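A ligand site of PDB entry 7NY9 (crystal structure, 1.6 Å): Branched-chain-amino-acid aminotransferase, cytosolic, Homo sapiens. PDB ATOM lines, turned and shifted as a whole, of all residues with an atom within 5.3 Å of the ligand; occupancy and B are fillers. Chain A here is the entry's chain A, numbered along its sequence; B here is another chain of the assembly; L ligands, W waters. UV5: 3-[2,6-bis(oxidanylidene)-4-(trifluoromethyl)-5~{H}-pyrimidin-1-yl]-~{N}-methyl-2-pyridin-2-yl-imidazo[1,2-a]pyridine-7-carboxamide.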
ATOM      1  N   PHE A  52      -7.478  -5.597  11.392  1.00  0.00           N
ATOM      2  CA  PHE A  52      -6.972  -6.092  10.085  1.00  0.00           C
ATOM      3  C   PHE A  52      -6.369  -7.493  10.236  1.00  0.00           C
ATOM      4  O   PHE A  52      -5.477  -7.680  11.077  1.00  0.00           O
ATOM      5  CB  PHE A  52      -5.907  -5.157   9.510  1.00  0.00           C
ATOM      6  CG  PHE A  52      -5.336  -5.627   8.199  1.00  0.00           C
ATOM      7  CD1 PHE A  52      -5.946  -5.304   7.002  1.00  0.00           C
ATOM      8  CD2 PHE A  52      -4.175  -6.393   8.160  1.00  0.00           C
ATOM      9  CE1 PHE A  52      -5.427  -5.744   5.798  1.00  0.00           C
ATOM     10  CE2 PHE A  52      -3.646  -6.824   6.953  1.00  0.00           C
ATOM     11  CZ  PHE A  52      -4.280  -6.501   5.775  1.00  0.00           C
ATOM     12  N   PHE A  98       3.084 -14.139  -1.376  1.00  0.00           N
ATOM     13  CA  PHE A  98       1.672 -13.844  -1.056  1.00  0.00           C
ATOM     14  C   PHE A  98       1.175 -12.738  -1.980  1.00  0.00           C
ATOM     15  O   PHE A  98       1.971 -12.089  -2.672  1.00  0.00           O
ATOM     16  CB  PHE A  98       1.504 -13.467   0.417  1.00  0.00           C
ATOM     17  CG  PHE A  98       2.140 -12.157   0.800  1.00  0.00           C
ATOM     18  CD1 PHE A  98       3.499 -12.067   1.044  1.00  0.00           C
ATOM     19  CD2 PHE A  98       1.374 -11.005   0.895  1.00  0.00           C
ATOM     20  CE1 PHE A  98       4.081 -10.862   1.390  1.00  0.00           C
ATOM     21  CE2 PHE A  98       1.951  -9.792   1.245  1.00  0.00           C
ATOM     22  CZ  PHE A  98       3.317  -9.727   1.498  1.00  0.00           C
ATOM     23  N   TYR A 164     -10.661  -8.825   2.721  1.00  0.00           N
ATOM     24  CA  TYR A 164      -9.252  -8.963   2.298  1.00  0.00           C
ATOM     25  C   TYR A 164      -9.036 -10.399   1.831  1.00  0.00           C
ATOM     26  O   TYR A 164      -9.423 -11.361   2.534  1.00  0.00           O
ATOM     27  CB  TYR A 164      -8.292  -8.570   3.420  1.00  0.00           C
ATOM     28  CG  TYR A 164      -6.849  -8.484   3.011  1.00  0.00           C
ATOM     29  CD1 TYR A 164      -6.374  -7.414   2.281  1.00  0.00           C
ATOM     30  CD2 TYR A 164      -5.935  -9.473   3.364  1.00  0.00           C
ATOM     31  CE1 TYR A 164      -5.042  -7.324   1.909  1.00  0.00           C
ATOM     32  CE2 TYR A 164      -4.608  -9.395   3.008  1.00  0.00           C
ATOM     33  CZ  TYR A 164      -4.144  -8.315   2.270  1.00  0.00           C
ATOM     34  OH  TYR A 164      -2.834  -8.215   1.925  1.00  0.00           O
ATOM     35  N   ARG A 166      -6.174 -13.135   0.586  1.00  0.00           N
ATOM     36  CA  ARG A 166      -4.749 -13.442   0.832  1.00  0.00           C
ATOM     37  C   ARG A 166      -4.409 -14.751   0.137  1.00  0.00           C
ATOM     38  O   ARG A 166      -4.398 -15.812   0.759  1.00  0.00           O
ATOM     39  CB  ARG A 166      -4.479 -13.463   2.338  1.00  0.00           C
ATOM     40  CG  ARG A 166      -3.104 -13.975   2.753  1.00  0.00           C
ATOM     41  CD  ARG A 166      -1.939 -13.354   2.011  1.00  0.00           C
ATOM     42  NE  ARG A 166      -1.794 -11.923   2.230  1.00  0.00           N
ATOM     43  CZ  ARG A 166      -1.078 -11.358   3.199  1.00  0.00           C
ATOM     44  NH1 ARG A 166      -0.432 -12.091   4.096  1.00  0.00           N
ATOM     45  NH2 ARG A 166      -1.024 -10.038   3.280  1.00  0.00           N
ATOM     46  N   TYR A 196      -8.781   1.640   7.315  1.00  0.00           N
ATOM     47  CA  TYR A 196      -7.340   1.518   7.680  1.00  0.00           C
ATOM     48  C   TYR A 196      -7.097   2.101   9.076  1.00  0.00           C
ATOM     49  O   TYR A 196      -6.434   1.424   9.917  1.00  0.00           O
ATOM     50  CB  TYR A 196      -6.449   2.207   6.643  1.00  0.00           C
ATOM     51  CG  TYR A 196      -4.975   1.995   6.855  1.00  0.00           C
ATOM     52  CD1 TYR A 196      -4.348   0.847   6.394  1.00  0.00           C
ATOM     53  CD2 TYR A 196      -4.200   2.925   7.508  1.00  0.00           C
ATOM     54  CE1 TYR A 196      -2.988   0.641   6.581  1.00  0.00           C
ATOM     55  CE2 TYR A 196      -2.845   2.732   7.715  1.00  0.00           C
ATOM     56  CZ  TYR A 196      -2.233   1.588   7.253  1.00  0.00           C
ATOM     57  OH  TYR A 196      -0.896   1.400   7.422  1.00  0.00           O
ATOM     58  N   LYS A 225       6.527  -9.901  -4.232  1.00  0.00           N
ATOM     59  CA  LYS A 225       5.823 -10.016  -2.937  1.00  0.00           C
ATOM     60  C   LYS A 225       6.206 -11.368  -2.323  1.00  0.00           C
ATOM     61  O   LYS A 225       5.327 -12.204  -2.042  1.00  0.00           O
ATOM     62  CB  LYS A 225       4.320  -9.791  -3.111  1.00  0.00           C
ATOM     63  CG  LYS A 225       3.752  -8.689  -2.219  1.00  0.00           C
ATOM     64  CD  LYS A 225       2.360  -8.263  -2.598  1.00  0.00           C
ATOM     65  CE  LYS A 225       1.714  -7.370  -1.572  1.00  0.00           C
ATOM     66  NZ  LYS A 225       2.537  -6.178  -1.261  1.00  0.00           N
ATOM     67  N   ALA A 236      13.144  -2.898  12.322  1.00  0.00           N
ATOM     68  CA  ALA A 236      13.070  -1.456  11.985  1.00  0.00           C
ATOM     69  C   ALA A 236      11.687  -0.913  12.371  1.00  0.00           C
ATOM     70  O   ALA A 236      11.612   0.224  12.866  1.00  0.00           O
ATOM     71  CB  ALA A 236      13.362  -1.233  10.511  1.00  0.00           C
ATOM     72  N   GLN A 237      10.612  -1.666  12.126  1.00  0.00           N
ATOM     73  CA  GLN A 237       9.233  -1.243  12.456  1.00  0.00           C
ATOM     74  C   GLN A 237       9.136  -1.033  13.967  1.00  0.00           C
ATOM     75  O   GLN A 237       8.575  -0.010  14.397  1.00  0.00           O
ATOM     76  CB  GLN A 237       8.194  -2.264  11.985  1.00  0.00           C
ATOM     77  CG  GLN A 237       8.090  -2.398  10.475  1.00  0.00           C
ATOM     78  CD  GLN A 237       7.035  -3.410  10.069  1.00  0.00           C
ATOM     79  OE1 GLN A 237       6.790  -3.627   8.888  1.00  0.00           O
ATOM     80  NE2 GLN A 237       6.404  -4.045  11.047  1.00  0.00           N
ATOM     81  N   CYS A 238       9.665  -1.967  14.759  1.00  0.00           N
ATOM     82  CA  CYS A 238       9.670  -1.855  16.241  1.00  0.00           C
ATOM     83  C   CYS A 238      10.431  -0.589  16.662  1.00  0.00           C
ATOM     84  O   CYS A 238       9.931   0.120  17.547  1.00  0.00           O
ATOM     85  CB  CYS A 238      10.277  -3.098  16.875  1.00  0.00           C
ATOM     86  SG  CYS A 238       9.189  -4.535  16.725  1.00  0.00           S
ATOM     87  N   ALA A 240      10.844   2.152  14.850  1.00  0.00           N
ATOM     88  CA  ALA A 240       9.940   3.247  14.435  1.00  0.00           C
ATOM     89  C   ALA A 240       8.925   3.524  15.550  1.00  0.00           C
ATOM     90  O   ALA A 240       8.850   4.686  16.024  1.00  0.00           O
ATOM     91  CB  ALA A 240       9.247   2.902  13.140  1.00  0.00           C
ATOM     92  N   VAL A 241       8.202   2.491  16.007  1.00  0.00           N
ATOM     93  CA  VAL A 241       7.138   2.639  17.033  1.00  0.00           C
ATOM     94  C   VAL A 241       7.774   3.106  18.348  1.00  0.00           C
ATOM     95  O   VAL A 241       7.160   3.961  19.008  1.00  0.00           O
ATOM     96  CB  VAL A 241       6.287   1.363  17.203  1.00  0.00           C
ATOM     97  CG1 VAL A 241       5.526   1.023  15.932  1.00  0.00           C
ATOM     98  CG2 VAL A 241       7.086   0.163  17.668  1.00  0.00           C
ATOM     99  N   GLN A 246       4.689   5.804  13.067  1.00  0.00           N
ATOM    100  CA  GLN A 246       3.688   4.760  12.701  1.00  0.00           C
ATOM    101  C   GLN A 246       4.246   3.867  11.591  1.00  0.00           C
ATOM    102  O   GLN A 246       3.792   2.721  11.491  1.00  0.00           O
ATOM    103  CB  GLN A 246       2.373   5.401  12.229  1.00  0.00           C
ATOM    104  CG  GLN A 246       1.577   6.050  13.347  1.00  0.00           C
ATOM    105  CD  GLN A 246       2.166   7.384  13.747  1.00  0.00           C
ATOM    106  OE1 GLN A 246       2.394   8.257  12.918  1.00  0.00           O
ATOM    107  NE2 GLN A 246       2.438   7.538  15.040  1.00  0.00           N
ATOM    108  N   GLN A 247       5.146   4.396  10.756  1.00  0.00           N
ATOM    109  CA  GLN A 247       5.690   3.638   9.599  1.00  0.00           C
ATOM    110  C   GLN A 247       7.198   3.911   9.460  1.00  0.00           C
ATOM    111  O   GLN A 247       7.662   4.953   9.950  1.00  0.00           O
ATOM    112  CB  GLN A 247       4.976   4.013   8.300  1.00  0.00           C
ATOM    113  CG  GLN A 247       3.451   3.924   8.339  1.00  0.00           C
ATOM    114  CD  GLN A 247       2.848   2.556   8.098  1.00  0.00           C
ATOM    115  OE1 GLN A 247       1.691   2.310   8.430  1.00  0.00           O
ATOM    116  NE2 GLN A 247       3.622   1.665   7.515  1.00  0.00           N
ATOM    117  N   VAL A 248       7.899   2.993   8.791  1.00  0.00           N
ATOM    118  CA  VAL A 248       9.316   3.150   8.388  1.00  0.00           C
ATOM    119  C   VAL A 248       9.356   3.853   7.034  1.00  0.00           C
ATOM    120  O   VAL A 248       8.629   3.409   6.134  1.00  0.00           O
ATOM    121  CB  VAL A 248      10.018   1.781   8.301  1.00  0.00           C
ATOM    122  CG1 VAL A 248      11.434   1.923   7.763  1.00  0.00           C
ATOM    123  CG2 VAL A 248       9.990   1.064   9.648  1.00  0.00           C
ATOM    124  N   GLY A 262       6.682   1.857   4.843  1.00  0.00           N
ATOM    125  CA  GLY A 262       6.237   0.562   5.388  1.00  0.00           C
ATOM    126  C   GLY A 262       6.044  -0.462   4.271  1.00  0.00           C
ATOM    127  O   GLY A 262       7.042  -0.837   3.630  1.00  0.00           O
ATOM    128  N   THR A 263       4.798  -0.855   4.020  1.00  0.00           N
ATOM    129  CA  THR A 263       4.432  -1.805   2.923  1.00  0.00           C
ATOM    130  C   THR A 263       3.624  -1.041   1.870  1.00  0.00           C
ATOM    131  O   THR A 263       2.683  -1.626   1.303  1.00  0.00           O
ATOM    132  CB  THR A 263       3.673  -3.020   3.444  1.00  0.00           C
ATOM    133  OG1 THR A 263       2.382  -2.567   3.854  1.00  0.00           O
ATOM    134  CG2 THR A 263       4.379  -3.731   4.583  1.00  0.00           C
ATOM    135  N   MET A 264       4.002   0.220   1.620  1.00  0.00           N
ATOM    136  CA  MET A 264       3.296   1.130   0.681  1.00  0.00           C
ATOM    137  C   MET A 264       4.275   1.824  -0.256  1.00  0.00           C
ATOM    138  O   MET A 264       5.384   2.191   0.165  1.00  0.00           O
ATOM    139  CB  MET A 264       2.513   2.211   1.442  1.00  0.00           C
ATOM    140  CG  MET A 264       1.376   1.641   2.264  1.00  0.00           C
ATOM    141  SD  MET A 264       0.347   2.904   3.015  1.00  0.00           S
ATOM    142  CE  MET A 264       1.309   3.262   4.485  1.00  0.00           C
ATOM    143  N   ALA A 337      -4.286  -1.826   1.519  1.00  0.00           N
ATOM    144  CA  ALA A 337      -4.827  -1.734   2.899  1.00  0.00           C
ATOM    145  C   ALA A 337      -5.286  -0.299   3.179  1.00  0.00           C
ATOM    146  O   ALA A 337      -6.401  -0.124   3.714  1.00  0.00           O
ATOM    147  CB  ALA A 337      -3.793  -2.204   3.902  1.00  0.00           C
ATOM    148  N   TYR B  93       5.438 -13.752   5.917  1.00  0.00           N
ATOM    149  CA  TYR B  93       6.462 -12.681   6.072  1.00  0.00           C
ATOM    150  C   TYR B  93       7.792 -13.271   6.520  1.00  0.00           C
ATOM    151  O   TYR B  93       8.645 -12.507   7.027  1.00  0.00           O
ATOM    152  CB  TYR B  93       5.935 -11.602   7.020  1.00  0.00           C
ATOM    153  CG  TYR B  93       4.547 -11.118   6.694  1.00  0.00           C
ATOM    154  CD1 TYR B  93       4.214 -10.709   5.403  1.00  0.00           C
ATOM    155  CD2 TYR B  93       3.536 -11.126   7.651  1.00  0.00           C
ATOM    156  CE1 TYR B  93       2.930 -10.299   5.090  1.00  0.00           C
ATOM    157  CE2 TYR B  93       2.254 -10.705   7.345  1.00  0.00           C
ATOM    158  CZ  TYR B  93       1.943 -10.296   6.060  1.00  0.00           C
ATOM    159  OH  TYR B  93       0.665  -9.918   5.763  1.00  0.00           O
ATOM    160  N   LEU B 176      -2.566 -11.535   9.753  1.00  0.00           N
ATOM    161  CA  LEU B 176      -1.915 -11.074   8.498  1.00  0.00           C
ATOM    162  C   LEU B 176      -1.240  -9.717   8.712  1.00  0.00           C
ATOM    163  O   LEU B 176      -0.655  -9.226   7.759  1.00  0.00           O
ATOM    164  CB  LEU B 176      -2.964 -11.009   7.385  1.00  0.00           C
ATOM    165  CG  LEU B 176      -3.732 -12.305   7.151  1.00  0.00           C
ATOM    166  CD1 LEU B 176      -4.650 -12.160   5.941  1.00  0.00           C
ATOM    167  CD2 LEU B 176      -2.781 -13.480   6.951  1.00  0.00           C
ATOM    168  N   GLY B 177      -1.311  -9.128   9.909  1.00  0.00           N
ATOM    169  CA  GLY B 177      -0.553  -7.890  10.186  1.00  0.00           C
ATOM    170  C   GLY B 177       0.947  -8.151  10.073  1.00  0.00           C
ATOM    171  O   GLY B 177       1.385  -9.218  10.551  1.00  0.00           O
ATOM    172  N   VAL B 178       1.700  -7.249   9.459  1.00  0.00           N
ATOM    173  CA  VAL B 178       3.191  -7.318   9.439  1.00  0.00           C
ATOM    174  C   VAL B 178       3.657  -6.785  10.794  1.00  0.00           C
ATOM    175  O   VAL B 178       3.672  -5.559  10.976  1.00  0.00           O
ATOM    176  CB  VAL B 178       3.795  -6.536   8.257  1.00  0.00           C
ATOM    177  CG1 VAL B 178       5.319  -6.544   8.301  1.00  0.00           C
ATOM    178  CG2 VAL B 178       3.310  -7.077   6.917  1.00  0.00           C
HETATM  179  N1  UV5 L   1       1.756  -1.947   8.260  1.00  0.00           N
HETATM  180  C4  UV5 L   1       2.897  -0.426   9.748  1.00  0.00           C
HETATM  181  C5  UV5 L   1       1.694  -1.006   9.280  1.00  0.00           C
HETATM  182  C6  UV5 L   1       5.489  -0.131   9.673  1.00  0.00           C
HETATM  183  C8  UV5 L   1      -0.380  -1.656   8.853  1.00  0.00           C
HETATM  184  C10 UV5 L   1      -1.759  -1.799   8.792  1.00  0.00           C
HETATM  185  C13 UV5 L   1      -4.492  -1.976   8.627  1.00  0.00           C
HETATM  186  C15 UV5 L   1      -2.337  -2.668   7.884  1.00  0.00           C
HETATM  187  C17 UV5 L   1       0.207  -4.640   7.236  1.00  0.00           C
HETATM  188  C21 UV5 L   1      -0.086  -2.813   5.669  1.00  0.00           C
HETATM  189  C24 UV5 L   1      -0.541  -5.913   3.697  1.00  0.00           C
HETATM  190  C28 UV5 L   1       2.989  -2.300   7.693  1.00  0.00           C
HETATM  191  C14 UV5 L   1      -3.717  -2.768   7.790  1.00  0.00           C
HETATM  192  C12 UV5 L   1      -3.860  -1.108   9.510  1.00  0.00           C
HETATM  193  N11 UV5 L   1      -2.540  -1.022   9.567  1.00  0.00           N
HETATM  194  N7  UV5 L   1       0.398  -0.854   9.605  1.00  0.00           N
HETATM  195  C3  UV5 L   1       4.148  -0.789   9.203  1.00  0.00           C
HETATM  196  O30 UV5 L   1       6.287   0.399   8.839  1.00  0.00           O
HETATM  197  N29 UV5 L   1       5.613   0.001  11.000  1.00  0.00           N
HETATM  198  C31 UV5 L   1       6.822   0.662  11.477  1.00  0.00           C
HETATM  199  C2  UV5 L   1       4.167  -1.731   8.172  1.00  0.00           C
HETATM  200  C9  UV5 L   1       0.450  -2.325   7.992  1.00  0.00           C
HETATM  201  N16 UV5 L   1       0.161  -3.266   6.970  1.00  0.00           N
HETATM  202  O22 UV5 L   1       0.432  -4.990   8.404  1.00  0.00           O
HETATM  203  C18 UV5 L   1      -0.028  -5.547   6.202  1.00  0.00           C
HETATM  204  C19 UV5 L   1      -0.269  -5.066   4.909  1.00  0.00           C
HETATM  205  F26 UV5 L   1      -0.499  -7.174   4.002  1.00  0.00           F
HETATM  206  F27 UV5 L   1      -1.775  -5.592   3.285  1.00  0.00           F
HETATM  207  F25 UV5 L   1       0.391  -5.630   2.774  1.00  0.00           F
HETATM  208  N20 UV5 L   1      -0.299  -3.714   4.657  1.00  0.00           N
HETATM  209  O23 UV5 L   1      -0.098  -1.620   5.411  1.00  0.00           O
HETATM  210  O   HOH W   1      -1.715  -3.334   0.826  1.00  0.00           O
HETATM  211  O   HOH W   2      -1.551  -4.392  10.838  1.00  0.00           O
HETATM  212  O   HOH W   3       7.703  -2.029   7.343  1.00  0.00           O
HETATM  213  O   HOH W   4       0.054  -1.896   1.956  1.00  0.00           O
HETATM  214  O   HOH W   5      -7.472  -1.741   9.739  1.00  0.00           O
HETATM  215  O   HOH W   6      -2.186  -6.035   0.627  1.00  0.00           O
HETATM  216  O   HOH W   7       2.668   0.032   5.587  1.00  0.00           O
HETATM  217  O   HOH W   8      -0.198   0.769  11.570  1.00  0.00           O
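The backbone NH of Val 248 sits at hydrogen-bond distance from an oxygen (O30) of the ligand (3.1 Å).
An oxygen (O22) of the ligand is in hydrogen-bond range of the backbone NH of Val 178 of chain B (2.8 Å).
NE2 of Gln 247 sits close to O30 of the ligand (3.2 Å).
OG1 of Thr 263 sits at hydrogen-bond distance from N20 of the ligand.
The side-chain hydroxyl (OH) of Tyr 196 is in hydrogen-bond range of a nitrogen (N7) of the ligand, at 3.4 Å.
The backbone carbonyl oxygen of Gln 246 is in hydrogen-bond range of a nitrogen (N29) of the ligand, at 3.3 Å.
Water W7 lies within hydrogen-bond range of NE2 of Gln 247 (2.7 Å), N of Thr 263 (2.8 Å) and O23 of the ligand (3.2 Å).
Water W3 lies within hydrogen-bond range of OE1 of Gln 237 and O30 of the ligand.
Water W4 bridges O of Thr 263 (2.7 Å) and N20 of the ligand (3.3 Å).
The guanidinium group (NH2) of Arg 166 is in hydrogen-bond range of the side-chain hydroxyl (OH) of Tyr 164, 2.9 Å away.
NH1 of Arg 166 lies within hydrogen-bond range of OH of Tyr 93 of chain B (3.0 Å).
O of Val 248 sits at hydrogen-bond distance from N of Gly 262, 2.8 Å away.
NE2 of Gln 237 sits at hydrogen-bond distance from O of Val 178 of chain B (3.1 Å).
The side-chain amide oxygen (OE1) of Gln 247 is in hydrogen-bond range of the side-chain hydroxyl (OH) of Tyr 196 (2.9 Å).
The side-chain hydroxyl (OH) of Tyr 93 of chain B is in hydrogen-bond range of the backbone carbonyl oxygen (O) of Leu 176 of chain B, 2.5 Å away.
OH of Tyr 164 lies close to F27 of the ligand (3.1 Å).
NH2 of Arg 166 sits close to F26 of the ligand (3.0 Å).
OH of Tyr 93 of chain B lies close to F26 of the ligand.
Residues that only touch the ligand: Phe 52 (3.3 Å), Gln 237 (3.2 Å), Ala 240 (3.7 Å), Gly 262 (3.5 Å), Ala 337 (3.9 Å) and Gly 177 of chain B (3.5 Å).
Hydrophobic or aromatic side chains within 4 Å of the ligand: Phe 52, Tyr 164, Tyr 196, Ala 240, Val 248, Ala 337 and Val 178 of chain B.
Within 4 Å of the ligand: Phe 52, Tyr 164, Arg 166, Tyr 196, Gln 237, Ala 240, Gln 246, Gln 247, Val 248, Gly 262, Thr 263, Ala 337, Tyr 93 of chain B, Gly 177 of chain B and Val 178 of chain B.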
